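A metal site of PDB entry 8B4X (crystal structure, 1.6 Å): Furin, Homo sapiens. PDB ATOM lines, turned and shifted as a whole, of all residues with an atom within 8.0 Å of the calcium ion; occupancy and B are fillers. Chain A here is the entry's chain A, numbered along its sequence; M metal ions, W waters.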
ATOM      1  N   LYS A  51      13.440  -7.367 -10.599  1.00  0.00           N
ATOM      2  CA  LYS A  51      13.978  -6.052 -10.240  1.00  0.00           C
ATOM      3  C   LYS A  51      13.164  -4.910 -10.829  1.00  0.00           C
ATOM      4  O   LYS A  51      13.283  -3.780 -10.356  1.00  0.00           O
ATOM      5  CB  LYS A  51      15.449  -5.951 -10.671  1.00  0.00           C
ATOM      6  CG  LYS A  51      15.693  -5.965 -12.156  1.00  0.00           C
ATOM      7  CD  LYS A  51      17.190  -6.112 -12.465  1.00  0.00           C
ATOM      8  CE  LYS A  51      17.442  -6.122 -13.972  1.00  0.00           C
ATOM      9  NZ  LYS A  51      16.801  -7.292 -14.631  1.00  0.00           N
ATOM     10  N   PHE A  66      23.227 -10.395  -7.549  1.00  0.00           N
ATOM     11  CA  PHE A  66      24.061 -11.162  -8.446  1.00  0.00           C
ATOM     12  C   PHE A  66      23.297 -12.411  -8.829  1.00  0.00           C
ATOM     13  O   PHE A  66      22.355 -12.826  -8.138  1.00  0.00           O
ATOM     14  CB  PHE A  66      25.421 -11.522  -7.816  1.00  0.00           C
ATOM     15  CG  PHE A  66      26.495 -11.761  -8.832  1.00  0.00           C
ATOM     16  CD1 PHE A  66      27.088 -10.692  -9.477  1.00  0.00           C
ATOM     17  CD2 PHE A  66      26.888 -13.044  -9.162  1.00  0.00           C
ATOM     18  CE1 PHE A  66      28.065 -10.902 -10.442  1.00  0.00           C
ATOM     19  CE2 PHE A  66      27.865 -13.254 -10.127  1.00  0.00           C
ATOM     20  CZ  PHE A  66      28.449 -12.182 -10.761  1.00  0.00           C
ATOM     21  N   ASP A  67      23.703 -13.011  -9.935  1.00  0.00           N
ATOM     22  CA  ASP A  67      23.139 -14.281 -10.399  1.00  0.00           C
ATOM     23  C   ASP A  67      24.273 -15.298 -10.333  1.00  0.00           C
ATOM     24  O   ASP A  67      25.111 -15.375 -11.240  1.00  0.00           O
ATOM     25  CB  ASP A  67      22.572 -14.143 -11.793  1.00  0.00           C
ATOM     26  CG  ASP A  67      21.945 -15.429 -12.315  1.00  0.00           C
ATOM     27  OD1 ASP A  67      22.144 -16.521 -11.741  1.00  0.00           O
ATOM     28  OD2 ASP A  67      21.251 -15.322 -13.337  1.00  0.00           O
ATOM     29  N   VAL A  68      24.299 -16.057  -9.239  1.00  0.00           N
ATOM     30  CA  VAL A  68      25.326 -17.072  -9.046  1.00  0.00           C
ATOM     31  C   VAL A  68      25.031 -18.302  -9.877  1.00  0.00           C
ATOM     32  O   VAL A  68      25.962 -18.991 -10.313  1.00  0.00           O
ATOM     33  CB  VAL A  68      25.437 -17.419  -7.553  1.00  0.00           C
ATOM     34  CG1 VAL A  68      26.428 -18.533  -7.329  1.00  0.00           C
ATOM     35  CG2 VAL A  68      25.850 -16.180  -6.767  1.00  0.00           C
ATOM     36  N   ASN A  69      23.753 -18.588 -10.141  1.00  0.00           N
ATOM     37  CA  ASN A  69      23.409 -19.770 -10.933  1.00  0.00           C
ATOM     38  C   ASN A  69      23.935 -19.667 -12.357  1.00  0.00           C
ATOM     39  O   ASN A  69      24.453 -20.645 -12.900  1.00  0.00           O
ATOM     40  CB  ASN A  69      21.888 -19.973 -10.961  1.00  0.00           C
ATOM     41  CG  ASN A  69      21.314 -20.399  -9.618  1.00  0.00           C
ATOM     42  OD1 ASN A  69      20.317 -19.836  -9.158  1.00  0.00           O
ATOM     43  ND2 ASN A  69      21.929 -21.393  -8.978  1.00  0.00           N
ATOM     44  N   ASP A  70      23.780 -18.501 -12.995  1.00  0.00           N
ATOM     45  CA  ASP A  70      24.205 -18.300 -14.383  1.00  0.00           C
ATOM     46  C   ASP A  70      25.476 -17.483 -14.500  1.00  0.00           C
ATOM     47  O   ASP A  70      25.944 -17.234 -15.619  1.00  0.00           O
ATOM     48  CB  ASP A  70      23.086 -17.616 -15.191  1.00  0.00           C
ATOM     49  CG  ASP A  70      21.995 -18.582 -15.638  1.00  0.00           C
ATOM     50  OD1 ASP A  70      22.175 -19.810 -15.478  1.00  0.00           O
ATOM     51  OD2 ASP A  70      20.960 -18.119 -16.167  1.00  0.00           O
ATOM     52  N   GLN A  71      26.036 -17.036 -13.379  1.00  0.00           N
ATOM     53  CA  GLN A  71      27.275 -16.257 -13.328  1.00  0.00           C
ATOM     54  C   GLN A  71      27.148 -14.976 -14.161  1.00  0.00           C
ATOM     55  O   GLN A  71      27.842 -14.769 -15.159  1.00  0.00           O
ATOM     56  CB  GLN A  71      28.476 -17.111 -13.777  1.00  0.00           C
ATOM     57  CG  GLN A  71      28.727 -18.346 -12.892  1.00  0.00           C
ATOM     58  CD  GLN A  71      29.943 -19.168 -13.329  1.00  0.00           C
ATOM     59  N   ASP A  72      26.236 -14.114 -13.727  1.00  0.00           N
ATOM     60  CA  ASP A  72      26.077 -12.787 -14.333  1.00  0.00           C
ATOM     61  C   ASP A  72      25.496 -11.869 -13.288  1.00  0.00           C
ATOM     62  O   ASP A  72      25.096 -12.316 -12.190  1.00  0.00           O
ATOM     63  CB  ASP A  72      25.213 -12.834 -15.605  1.00  0.00           C
ATOM     64  CG  ASP A  72      23.739 -13.147 -15.336  1.00  0.00           C
ATOM     65  OD1 ASP A  72      23.046 -12.345 -14.676  1.00  0.00           O
ATOM     66  OD2 ASP A  72      23.238 -14.185 -15.841  1.00  0.00           O
ATOM     67  N   PRO A  73      25.455 -10.558 -13.548  1.00  0.00           N
ATOM     68  CA  PRO A  73      25.056  -9.608 -12.501  1.00  0.00           C
ATOM     69  C   PRO A  73      23.563  -9.501 -12.300  1.00  0.00           C
ATOM     70  O   PRO A  73      23.134  -8.910 -11.306  1.00  0.00           O
ATOM     71  CB  PRO A  73      25.627  -8.265 -12.996  1.00  0.00           C
ATOM     72  CG  PRO A  73      26.565  -8.614 -14.102  1.00  0.00           C
ATOM     73  CD  PRO A  73      26.005  -9.858 -14.724  1.00  0.00           C
ATOM     74  N   ASP A  74      22.759 -10.083 -13.202  1.00  0.00           N
ATOM     75  CA  ASP A  74      21.335  -9.795 -13.288  1.00  0.00           C
ATOM     76  C   ASP A  74      20.525 -10.906 -12.642  1.00  0.00           C
ATOM     77  O   ASP A  74      20.447 -12.007 -13.205  1.00  0.00           O
ATOM     78  CB  ASP A  74      20.948  -9.619 -14.751  1.00  0.00           C
ATOM     79  CG  ASP A  74      19.474  -9.337 -14.965  1.00  0.00           C
ATOM     80  OD1 ASP A  74      18.683  -9.367 -13.983  1.00  0.00           O
ATOM     81  OD2 ASP A  74      19.099  -9.085 -16.116  1.00  0.00           O
ATOM     82  N   PRO A  75      19.890 -10.658 -11.483  1.00  0.00           N
ATOM     83  CA  PRO A  75      19.204 -11.737 -10.761  1.00  0.00           C
ATOM     84  C   PRO A  75      17.756 -11.958 -11.182  1.00  0.00           C
ATOM     85  O   PRO A  75      16.984 -12.555 -10.421  1.00  0.00           O
ATOM     86  CB  PRO A  75      19.252 -11.243  -9.317  1.00  0.00           C
ATOM     87  CG  PRO A  75      18.949  -9.761  -9.512  1.00  0.00           C
ATOM     88  CD  PRO A  75      19.803  -9.389 -10.734  1.00  0.00           C
ATOM     89  N   GLN A  76      17.380 -11.457 -12.348  1.00  0.00           N
ATOM     90  CA  GLN A  76      16.007 -11.600 -12.787  1.00  0.00           C
ATOM     91  C   GLN A  76      15.591 -13.073 -12.722  1.00  0.00           C
ATOM     92  O   GLN A  76      16.359 -13.943 -13.143  1.00  0.00           O
ATOM     93  CB  GLN A  76      15.841 -11.104 -14.232  1.00  0.00           C
ATOM     94  CG  GLN A  76      14.398 -10.920 -14.646  1.00  0.00           C
ATOM     95  CD  GLN A  76      13.782  -9.659 -14.078  1.00  0.00           C
ATOM     96  OE1 GLN A  76      14.486  -8.748 -13.636  1.00  0.00           O
ATOM     97  NE2 GLN A  76      12.454  -9.593 -14.077  1.00  0.00           N
ATOM     98  N   PRO A  77      14.407 -13.374 -12.200  1.00  0.00           N
ATOM     99  CA  PRO A  77      13.974 -14.773 -12.163  1.00  0.00           C
ATOM    100  C   PRO A  77      13.749 -15.353 -13.559  1.00  0.00           C
ATOM    101  O   PRO A  77      13.465 -14.642 -14.522  1.00  0.00           O
ATOM    102  CB  PRO A  77      12.649 -14.733 -11.374  1.00  0.00           C
ATOM    103  CG  PRO A  77      12.619 -13.411 -10.708  1.00  0.00           C
ATOM    104  CD  PRO A  77      13.414 -12.479 -11.596  1.00  0.00           C
ATOM    105  N   ARG A  78      13.868 -16.675 -13.621  1.00  0.00           N
ATOM    106  CA  ARG A  78      13.529 -17.466 -14.796  1.00  0.00           C
ATOM    107  C   ARG A  78      12.025 -17.735 -14.807  1.00  0.00           C
ATOM    108  O   ARG A  78      11.487 -18.323 -13.869  1.00  0.00           O
ATOM    109  CB  ARG A  78      14.324 -18.776 -14.782  1.00  0.00           C
ATOM    110  CG  ARG A  78      14.046 -19.747 -15.951  1.00  0.00           C
ATOM    111  CD  ARG A  78      14.995 -20.961 -15.913  1.00  0.00           C
ATOM    112  NE  ARG A  78      14.820 -21.720 -14.685  1.00  0.00           N
ATOM    113  CZ  ARG A  78      13.913 -22.675 -14.489  1.00  0.00           C
ATOM    114  NH1 ARG A  78      13.133 -23.101 -15.480  1.00  0.00           N
ATOM    115  NH2 ARG A  78      13.777 -23.209 -13.281  1.00  0.00           N
ATOM    116  N   ARG A 118      20.386 -14.641  -7.125  1.00  0.00           N
ATOM    117  CA  ARG A 118      19.754 -15.784  -7.784  1.00  0.00           C
ATOM    118  C   ARG A 118      20.714 -16.947  -7.590  1.00  0.00           C
ATOM    119  O   ARG A 118      21.762 -17.012  -8.235  1.00  0.00           O
ATOM    120  CB  ARG A 118      19.484 -15.492  -9.251  1.00  0.00           C
ATOM    121  CG  ARG A 118      18.837 -16.660  -9.992  1.00  0.00           C
ATOM    122  CD  ARG A 118      18.362 -16.240 -11.380  1.00  0.00           C
ATOM    123  NE  ARG A 118      17.806 -17.367 -12.112  1.00  0.00           N
ATOM    124  CZ  ARG A 118      18.455 -18.045 -13.053  1.00  0.00           C
ATOM    125  NH1 ARG A 118      19.644 -17.662 -13.492  1.00  0.00           N
ATOM    126  NH2 ARG A 118      17.893 -19.136 -13.573  1.00  0.00           N
HETATM  127 CA    CA M   1      20.916 -13.662 -14.931  1.00  0.00          CA
HETATM  128  O   HOH W   1      20.512 -12.322 -16.893  1.00  0.00           O
HETATM  129  O   HOH W   2      18.535 -13.831 -14.815  1.00  0.00           O
HETATM  130  O   HOH W   3      20.461 -15.418 -16.495  1.00  0.00           O
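The calcium ion is bound by OD2 of Asp 67 (2.3 Å), water W2 (2.4 Å), water W3 (2.4 Å), water W1 (2.4 Å), O of Asp 74 (2.4 Å), OD1 of Asp 72 (2.5 Å) and OD2 of Asp 72 (2.5 Å).
The calcium ion has seven donor atoms within binding distance.
The nearest printed residue that does not touch the calcium ion is Arg 118 (4.4 Å).
NZ of Lys 51 is in salt-bridge range of OD1 of Asp 74, at 2.9 Å.
The side-chain carboxylate (OD1) of Asp 74 sits at hydrogen-bond distance from the backbone NH (N) of Gln 76 (3.0 Å).
OD1 of Asp 67 is in hydrogen-bond range of N of Asn 69 (3.1 Å).
The guanidinium group (NH1) of Arg 118 is in salt-bridge range of the side-chain carboxylate (OD1) of Asp 67, at 3.3 Å.
The backbone NH (N) of Asp 70 is in hydrogen-bond range of the side-chain carboxylate (OD1) of Asp 67 (2.9 Å).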
